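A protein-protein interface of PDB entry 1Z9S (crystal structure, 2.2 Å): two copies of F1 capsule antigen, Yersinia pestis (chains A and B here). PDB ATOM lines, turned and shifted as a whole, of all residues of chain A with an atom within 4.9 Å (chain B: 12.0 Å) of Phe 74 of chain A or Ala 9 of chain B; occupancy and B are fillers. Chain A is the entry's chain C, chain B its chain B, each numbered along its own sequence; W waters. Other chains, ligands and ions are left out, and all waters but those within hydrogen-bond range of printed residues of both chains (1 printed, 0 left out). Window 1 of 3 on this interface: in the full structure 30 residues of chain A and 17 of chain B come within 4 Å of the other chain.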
ATOM      1  N   TYR A  23     -24.810  -7.880  15.065  1.00  0.00           N
ATOM      2  CA  TYR A  23     -23.686  -8.774  14.831  1.00  0.00           C
ATOM      3  C   TYR A  23     -22.404  -8.230  15.454  1.00  0.00           C
ATOM      4  O   TYR A  23     -22.164  -7.021  15.455  1.00  0.00           O
ATOM      5  CB  TYR A  23     -23.479  -8.937  13.322  1.00  0.00           C
ATOM      6  CG  TYR A  23     -22.333  -9.841  12.942  1.00  0.00           C
ATOM      7  CD1 TYR A  23     -22.501 -11.225  12.893  1.00  0.00           C
ATOM      8  CD2 TYR A  23     -21.074  -9.314  12.629  1.00  0.00           C
ATOM      9  CE1 TYR A  23     -21.453 -12.068  12.536  1.00  0.00           C
ATOM     10  CE2 TYR A  23     -20.013 -10.153  12.273  1.00  0.00           C
ATOM     11  CZ  TYR A  23     -20.212 -11.530  12.224  1.00  0.00           C
ATOM     12  OH  TYR A  23     -19.189 -12.372  11.836  1.00  0.00           O
ATOM     13  N   VAL A  43     -16.545 -17.144  13.852  1.00  0.00           N
ATOM     14  CA  VAL A  43     -16.437 -16.030  12.911  1.00  0.00           C
ATOM     15  C   VAL A  43     -17.026 -14.738  13.476  1.00  0.00           C
ATOM     16  O   VAL A  43     -16.496 -13.639  13.257  1.00  0.00           O
ATOM     17  CB  VAL A  43     -17.178 -16.353  11.596  1.00  0.00           C
ATOM     18  CG1 VAL A  43     -16.968 -15.239  10.596  1.00  0.00           C
ATOM     19  CG2 VAL A  43     -16.676 -17.688  11.034  1.00  0.00           C
ATOM     20  N   LEU A  72     -24.258 -19.736   5.615  1.00  0.00           N
ATOM     21  CA  LEU A  72     -24.172 -18.305   5.351  1.00  0.00           C
ATOM     22  C   LEU A  72     -22.824 -18.212   4.641  1.00  0.00           C
ATOM     23  O   LEU A  72     -21.805 -18.673   5.165  1.00  0.00           O
ATOM     24  CB  LEU A  72     -24.151 -17.489   6.647  1.00  0.00           C
ATOM     25  CG  LEU A  72     -25.482 -17.357   7.406  1.00  0.00           C
ATOM     26  CD1 LEU A  72     -25.320 -16.400   8.572  1.00  0.00           C
ATOM     27  CD2 LEU A  72     -26.552 -16.837   6.461  1.00  0.00           C
ATOM     28  N   THR A  73     -22.827 -17.649   3.441  1.00  0.00           N
ATOM     29  CA  THR A  73     -21.619 -17.523   2.629  1.00  0.00           C
ATOM     30  C   THR A  73     -20.985 -16.134   2.753  1.00  0.00           C
ATOM     31  O   THR A  73     -21.675 -15.117   2.594  1.00  0.00           O
ATOM     32  CB  THR A  73     -21.962 -17.792   1.147  1.00  0.00           C
ATOM     33  OG1 THR A  73     -22.605 -19.066   1.040  1.00  0.00           O
ATOM     34  CG2 THR A  73     -20.707 -17.800   0.280  1.00  0.00           C
ATOM     35  N   PHE A  74     -19.686 -16.096   3.059  1.00  0.00           N
ATOM     36  CA  PHE A  74     -18.958 -14.832   3.191  1.00  0.00           C
ATOM     37  C   PHE A  74     -18.126 -14.601   1.941  1.00  0.00           C
ATOM     38  O   PHE A  74     -17.550 -15.546   1.389  1.00  0.00           O
ATOM     39  CB  PHE A  74     -18.048 -14.841   4.423  1.00  0.00           C
ATOM     40  CG  PHE A  74     -18.790 -14.704   5.731  1.00  0.00           C
ATOM     41  CD1 PHE A  74     -19.656 -15.701   6.162  1.00  0.00           C
ATOM     42  CD2 PHE A  74     -18.614 -13.574   6.526  1.00  0.00           C
ATOM     43  CE1 PHE A  74     -20.349 -15.579   7.378  1.00  0.00           C
ATOM     44  CE2 PHE A  74     -19.295 -13.438   7.739  1.00  0.00           C
ATOM     45  CZ  PHE A  74     -20.170 -14.449   8.168  1.00  0.00           C
ATOM     46  N   THR A  75     -18.036 -13.345   1.514  1.00  0.00           N
ATOM     47  CA  THR A  75     -17.303 -13.015   0.291  1.00  0.00           C
ATOM     48  C   THR A  75     -16.246 -11.915   0.403  1.00  0.00           C
ATOM     49  O   THR A  75     -16.407 -10.945   1.147  1.00  0.00           O
ATOM     50  CB  THR A  75     -18.288 -12.598  -0.814  1.00  0.00           C
ATOM     51  OG1 THR A  75     -19.261 -13.632  -0.994  1.00  0.00           O
ATOM     52  CG2 THR A  75     -17.551 -12.364  -2.130  1.00  0.00           C
ATOM     53  N   SER A  76     -15.169 -12.074  -0.360  1.00  0.00           N
ATOM     54  CA  SER A  76     -14.090 -11.092  -0.383  1.00  0.00           C
ATOM     55  C   SER A  76     -14.609  -9.802  -1.018  1.00  0.00           C
ATOM     56  O   SER A  76     -15.647  -9.802  -1.685  1.00  0.00           O
ATOM     57  CB  SER A  76     -12.890 -11.631  -1.174  1.00  0.00           C
ATOM     58  OG  SER A  76     -13.228 -11.899  -2.524  1.00  0.00           O
ATOM     59  N   HIS A  82     -13.664 -14.426  -3.516  1.00  0.00           N
ATOM     60  CA  HIS A  82     -13.165 -15.524  -2.695  1.00  0.00           C
ATOM     61  C   HIS A  82     -14.309 -15.728  -1.710  1.00  0.00           C
ATOM     62  O   HIS A  82     -14.849 -14.758  -1.196  1.00  0.00           O
ATOM     63  CB  HIS A  82     -11.903 -15.110  -1.927  1.00  0.00           C
ATOM     64  CG  HIS A  82     -10.712 -14.868  -2.801  1.00  0.00           C
ATOM     65  ND1 HIS A  82     -10.229 -15.817  -3.677  1.00  0.00           N
ATOM     66  CD2 HIS A  82      -9.922 -13.780  -2.954  1.00  0.00           C
ATOM     67  CE1 HIS A  82      -9.194 -15.322  -4.332  1.00  0.00           C
ATOM     68  NE2 HIS A  82      -8.985 -14.087  -3.912  1.00  0.00           N
ATOM     69  N   GLN A  83     -14.683 -16.972  -1.441  1.00  0.00           N
ATOM     70  CA  GLN A  83     -15.790 -17.229  -0.526  1.00  0.00           C
ATOM     71  C   GLN A  83     -15.548 -18.417   0.399  1.00  0.00           C
ATOM     72  O   GLN A  83     -14.817 -19.346   0.063  1.00  0.00           O
ATOM     73  CB  GLN A  83     -17.082 -17.498  -1.320  1.00  0.00           C
ATOM     74  CG  GLN A  83     -17.563 -16.372  -2.222  1.00  0.00           C
ATOM     75  CD  GLN A  83     -18.891 -16.692  -2.895  1.00  0.00           C
ATOM     76  OE1 GLN A  83     -18.979 -17.597  -3.723  1.00  0.00           O
ATOM     77  NE2 GLN A  83     -19.936 -15.948  -2.532  1.00  0.00           N
ATOM     78  N   PHE A  84     -16.164 -18.372   1.571  1.00  0.00           N
ATOM     79  CA  PHE A  84     -16.090 -19.464   2.534  1.00  0.00           C
ATOM     80  C   PHE A  84     -17.471 -19.529   3.165  1.00  0.00           C
ATOM     81  O   PHE A  84     -18.180 -18.520   3.241  1.00  0.00           O
ATOM     82  CB  PHE A  84     -14.973 -19.252   3.594  1.00  0.00           C
ATOM     83  CG  PHE A  84     -15.202 -18.098   4.552  1.00  0.00           C
ATOM     84  CD1 PHE A  84     -15.940 -18.274   5.724  1.00  0.00           C
ATOM     85  CD2 PHE A  84     -14.597 -16.863   4.329  1.00  0.00           C
ATOM     86  CE1 PHE A  84     -16.065 -17.233   6.668  1.00  0.00           C
ATOM     87  CE2 PHE A  84     -14.712 -15.821   5.253  1.00  0.00           C
ATOM     88  CZ  PHE A  84     -15.448 -16.007   6.429  1.00  0.00           C
ATOM     89  N   THR A  86     -20.150 -20.910   6.369  1.00  0.00           N
ATOM     90  CA  THR A  86     -20.222 -21.033   7.815  1.00  0.00           C
ATOM     91  C   THR A  86     -21.582 -21.636   8.152  1.00  0.00           C
ATOM     92  O   THR A  86     -22.422 -21.801   7.274  1.00  0.00           O
ATOM     93  CB  THR A  86     -20.170 -19.658   8.483  1.00  0.00           C
ATOM     94  OG1 THR A  86     -21.312 -18.896   8.070  1.00  0.00           O
ATOM     95  CG2 THR A  86     -18.909 -18.918   8.100  1.00  0.00           C
ATOM     96  N   VAL A 123     -21.717 -17.935  14.500  1.00  0.00           N
ATOM     97  CA  VAL A 123     -21.404 -18.209  13.106  1.00  0.00           C
ATOM     98  C   VAL A 123     -20.089 -18.970  13.177  1.00  0.00           C
ATOM     99  O   VAL A 123     -19.041 -18.399  13.500  1.00  0.00           O
ATOM    100  CB  VAL A 123     -21.229 -16.900  12.309  1.00  0.00           C
ATOM    101  CG1 VAL A 123     -20.758 -17.203  10.878  1.00  0.00           C
ATOM    102  CG2 VAL A 123     -22.560 -16.144  12.274  1.00  0.00           C
ATOM    103  N   TYR A 138     -14.102  -9.788   4.718  1.00  0.00           N
ATOM    104  CA  TYR A 138     -15.163 -10.579   4.096  1.00  0.00           C
ATOM    105  C   TYR A 138     -16.491 -10.155   4.703  1.00  0.00           C
ATOM    106  O   TYR A 138     -16.545  -9.782   5.876  1.00  0.00           O
ATOM    107  CB  TYR A 138     -14.929 -12.072   4.353  1.00  0.00           C
ATOM    108  CG  TYR A 138     -13.844 -12.671   3.494  1.00  0.00           C
ATOM    109  CD1 TYR A 138     -12.512 -12.300   3.659  1.00  0.00           C
ATOM    110  CD2 TYR A 138     -14.153 -13.600   2.495  1.00  0.00           C
ATOM    111  CE1 TYR A 138     -11.506 -12.836   2.851  1.00  0.00           C
ATOM    112  CE2 TYR A 138     -13.151 -14.142   1.681  1.00  0.00           C
ATOM    113  CZ  TYR A 138     -11.832 -13.756   1.866  1.00  0.00           C
ATOM    114  OH  TYR A 138     -10.833 -14.295   1.073  1.00  0.00           O
ATOM    115  N   THR A 139     -17.561 -10.211   3.919  1.00  0.00           N
ATOM    116  CA  THR A 139     -18.870  -9.814   4.425  1.00  0.00           C
ATOM    117  C   THR A 139     -19.973 -10.698   3.873  1.00  0.00           C
ATOM    118  O   THR A 139     -19.768 -11.467   2.938  1.00  0.00           O
ATOM    119  CB  THR A 139     -19.229  -8.366   4.027  1.00  0.00           C
ATOM    120  OG1 THR A 139     -19.329  -8.280   2.597  1.00  0.00           O
ATOM    121  CG2 THR A 139     -18.162  -7.391   4.502  1.00  0.00           C
ATOM    122  N   ASP A 140     -21.149 -10.564   4.467  1.00  0.00           N
ATOM    123  CA  ASP A 140     -22.332 -11.289   4.039  1.00  0.00           C
ATOM    124  C   ASP A 140     -23.500 -10.476   4.576  1.00  0.00           C
ATOM    125  O   ASP A 140     -23.642 -10.309   5.785  1.00  0.00           O
ATOM    126  CB  ASP A 140     -22.346 -12.710   4.617  1.00  0.00           C
ATOM    127  CG  ASP A 140     -23.493 -13.560   4.068  1.00  0.00           C
ATOM    128  OD1 ASP A 140     -23.831 -13.410   2.870  1.00  0.00           O
ATOM    129  OD2 ASP A 140     -24.046 -14.391   4.836  1.00  0.00           O
ATOM    130  N   VAL A 142     -26.827 -10.210   5.746  1.00  0.00           N
ATOM    131  CA  VAL A 142     -27.774 -11.182   6.268  1.00  0.00           C
ATOM    132  C   VAL A 142     -29.159 -10.637   6.588  1.00  0.00           C
ATOM    133  O   VAL A 142     -29.320  -9.463   6.936  1.00  0.00           O
ATOM    134  CB  VAL A 142     -27.202 -11.853   7.544  1.00  0.00           C
ATOM    135  CG1 VAL A 142     -28.138 -12.955   8.035  1.00  0.00           C
ATOM    136  CG2 VAL A 142     -25.814 -12.429   7.249  1.00  0.00           C
ATOM    137  N   ALA B   5     -35.584  -8.616  10.131  1.00  0.00           N
ATOM    138  CA  ALA B   5     -34.541  -7.684  10.520  1.00  0.00           C
ATOM    139  C   ALA B   5     -33.330  -8.112   9.702  1.00  0.00           C
ATOM    140  O   ALA B   5     -33.235  -9.270   9.290  1.00  0.00           O
ATOM    141  CB  ALA B   5     -34.250  -7.796  12.016  1.00  0.00           C
ATOM    142  N   SER B   6     -32.409  -7.189   9.454  1.00  0.00           N
ATOM    143  CA  SER B   6     -31.225  -7.529   8.675  1.00  0.00           C
ATOM    144  C   SER B   6     -29.993  -6.850   9.243  1.00  0.00           C
ATOM    145  O   SER B   6     -30.089  -5.858   9.970  1.00  0.00           O
ATOM    146  CB  SER B   6     -31.402  -7.101   7.227  1.00  0.00           C
ATOM    147  OG  SER B   6     -31.420  -5.691   7.155  1.00  0.00           O
ATOM    148  N   THR B   7     -28.832  -7.393   8.903  1.00  0.00           N
ATOM    149  CA  THR B   7     -27.572  -6.849   9.372  1.00  0.00           C
ATOM    150  C   THR B   7     -26.457  -7.320   8.454  1.00  0.00           C
ATOM    151  O   THR B   7     -26.694  -8.077   7.518  1.00  0.00           O
ATOM    152  CB  THR B   7     -27.272  -7.316  10.814  1.00  0.00           C
ATOM    153  OG1 THR B   7     -26.104  -6.644  11.300  1.00  0.00           O
ATOM    154  CG2 THR B   7     -27.038  -8.816  10.854  1.00  0.00           C
ATOM    155  N   THR B   8     -25.242  -6.863   8.709  1.00  0.00           N
ATOM    156  CA  THR B   8     -24.114  -7.280   7.890  1.00  0.00           C
ATOM    157  C   THR B   8     -23.132  -8.062   8.751  1.00  0.00           C
ATOM    158  O   THR B   8     -22.693  -7.582   9.792  1.00  0.00           O
ATOM    159  CB  THR B   8     -23.392  -6.066   7.253  1.00  0.00           C
ATOM    160  OG1 THR B   8     -24.339  -5.280   6.514  1.00  0.00           O
ATOM    161  CG2 THR B   8     -22.304  -6.539   6.287  1.00  0.00           C
ATOM    162  N   ALA B   9     -22.815  -9.281   8.333  1.00  0.00           N
ATOM    163  CA  ALA B   9     -21.870 -10.099   9.081  1.00  0.00           C
ATOM    164  C   ALA B   9     -20.507  -9.816   8.483  1.00  0.00           C
ATOM    165  O   ALA B   9     -20.381  -9.671   7.272  1.00  0.00           O
ATOM    166  CB  ALA B   9     -22.213 -11.584   8.938  1.00  0.00           C
ATOM    167  N   THR B  10     -19.487  -9.734   9.321  1.00  0.00           N
ATOM    168  CA  THR B  10     -18.153  -9.450   8.823  1.00  0.00           C
ATOM    169  C   THR B  10     -17.155 -10.439   9.381  1.00  0.00           C
ATOM    170  O   THR B  10     -17.408 -11.089  10.390  1.00  0.00           O
ATOM    171  CB  THR B  10     -17.715  -8.037   9.220  1.00  0.00           C
ATOM    172  OG1 THR B  10     -17.783  -7.912  10.644  1.00  0.00           O
ATOM    173  CG2 THR B  10     -18.632  -6.993   8.580  1.00  0.00           C
ATOM    174  N   ALA B  11     -16.010 -10.535   8.714  1.00  0.00           N
ATOM    175  CA  ALA B  11     -14.942 -11.439   9.114  1.00  0.00           C
ATOM    176  C   ALA B  11     -13.652 -10.856   8.559  1.00  0.00           C
ATOM    177  O   ALA B  11     -13.656 -10.279   7.475  1.00  0.00           O
ATOM    178  CB  ALA B  11     -15.178 -12.821   8.523  1.00  0.00           C
ATOM    179  N   THR B  12     -12.560 -11.006   9.297  1.00  0.00           N
ATOM    180  CA  THR B  12     -11.266 -10.486   8.863  1.00  0.00           C
ATOM    181  C   THR B  12     -10.322 -11.674   8.747  1.00  0.00           C
ATOM    182  O   THR B  12     -10.048 -12.343   9.741  1.00  0.00           O
ATOM    183  CB  THR B  12     -10.695  -9.464   9.905  1.00  0.00           C
ATOM    184  OG1 THR B  12     -11.612  -8.363  10.050  1.00  0.00           O
ATOM    185  CG2 THR B  12      -9.328  -8.928   9.463  1.00  0.00           C
ATOM    186  N   LEU B  13      -9.855 -11.966   7.536  1.00  0.00           N
ATOM    187  CA  LEU B  13      -8.940 -13.083   7.358  1.00  0.00           C
ATOM    188  C   LEU B  13      -7.517 -12.546   7.206  1.00  0.00           C
ATOM    189  O   LEU B  13      -7.298 -11.537   6.518  1.00  0.00           O
ATOM    190  CB  LEU B  13      -9.310 -13.914   6.128  1.00  0.00           C
ATOM    191  CG  LEU B  13     -10.737 -14.411   5.860  1.00  0.00           C
ATOM    192  CD1 LEU B  13     -10.613 -15.763   5.172  1.00  0.00           C
ATOM    193  CD2 LEU B  13     -11.585 -14.525   7.130  1.00  0.00           C
HETATM  194  O   HOH W   1     -28.444  -7.342   5.458  1.00  0.00           O
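Val 43 of chain A touches just these residues of chain B: Thr 10 and Ala 11. No residue of chain B comes within 4 Å of Leu 72 of chain A. No residue of chain B comes within 4 Å of Ser 76 of chain A. No residue of chain B comes within 4 Å of Gln 83 of chain A. Of chain B, only Ala 11 (3.8 Å) and Leu 13 (3.9 Å) come within 4 Å of Phe 84 of chain A. No residue of chain B comes within 4 Å of Thr 86 of chain A. No residue of chain B comes within 4 Å of Val 123 of chain A. Of chain B, only Ala 9 (3.2 Å) comes within 4 Å of Thr 139 of chain A. Asp 140 of chain A touches just these residues of chain B: Thr 8 and Ala 9. Val 142 of chain A touches two residues of chain B. Of the printed residues of chain A, Ser 6 of chain B touches Val 142 (3.2 Å). Of the printed residues of chain A, Thr 8 of chain B touches Tyr 23 and Asp 140. Of chain A, only Tyr 23, Phe 74, Thr 139 and Asp 140 come within 4 Å of Ala 9 of chain B. Of the printed residues of chain A, Thr 10 of chain B touches Tyr 23, Val 43 and Tyr 138. Printed residues of chain A within 4 Å of Ala 11 of chain B: Val 43 (3.7 Å), Phe 84 (3.8 Å) and Tyr 138 (2.8 Å). Printed residues of chain A within 4 Å of Leu 13 of chain B: Phe 84 (3.9 Å) and Tyr 138 (3.5 Å). The nearest printed residue of chain B that does not touch Phe 74 of chain A is Thr 10 of chain B (4.01 Å).
Among the printed residues, pairs that only touch across the chains: Val 142 of chain A with Ser 6 of chain B, Thr 139 of chain A with Ala 9 of chain B, Tyr 138 of chain A with Thr 10 of chain B, Tyr 138 of chain A with Leu 13 of chain B, Phe 74 of chain A with Ala 9 of chain B, Val 43 of chain A with Ala 11 of chain B, Tyr 23 of chain A with Ala 9 of chain B, Tyr 23 of chain A with Thr 8 of chain B, Asp 140 of chain A with Thr 8 of chain B, Phe 84 of chain A with Ala 11 of chain B, Phe 84 of chain A with Leu 13 of chain B and Val 43 of chain A with Thr 10 of chain B.
Water W1 lies within hydrogen-bond range of O of Val 142 of chain A (2.7 Å) and O of Thr 7 of chain B (2.8 Å).
Hydrophobic or aromatic side chains of chain B that line the printed part of chain A: Ala 9, Ala 11 and Leu 13. Along chain B the printed residues that touch a printed residue of chain A span positions 6 to 13. Hydrophobic or aromatic side chains of chain A that line the printed part of chain B: Tyr 23, Val 43, Phe 74, Phe 84, Tyr 138 and Val 142. Among the printed residues, no Asp or Glu carboxylate lies within 4 Å of a Lys or Arg side-chain nitrogen of the other chain.
O of Thr 7 of chain B lies within hydrogen-bond range of N of Val 142 of chain A (2.8 Å). The backbone NH of Ala 9 of chain B is in hydrogen-bond range of the backbone carbonyl oxygen of Asp 140 of chain A, at 2.9 Å. The side-chain hydroxyl of Tyr 23 of chain A sits at hydrogen-bond distance from the backbone carbonyl oxygen of Thr 10 of chain B (2.6 Å). The backbone carbonyl oxygen (O) of Ala 11 of chain B is in hydrogen-bond range of the backbone NH (N) of Tyr 138 of chain A (2.8 Å).
No position is printed for both chains. Of the 16 pairs that touch across the chains among the printed residues, none has its exchanged pair printed and touching as well.
The backbone carbonyl oxygen (O) of Val 43 of chain A is in hydrogen-bond range of the side-chain hydroxyl (OH) of Tyr 23 of chain A (3.3 Å). The backbone NH (N) of Val 43 of chain A lies within hydrogen-bond range of the backbone carbonyl oxygen (O) of Val 123 of chain A, 2.8 Å away. N of Phe 74 of chain A sits at hydrogen-bond distance from O of Phe 84 of chain A (2.9 Å). The backbone carbonyl oxygen (O) of Thr 139 of chain A lies within hydrogen-bond range of the backbone NH (N) of Thr 75 of chain A, at 2.9 Å.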
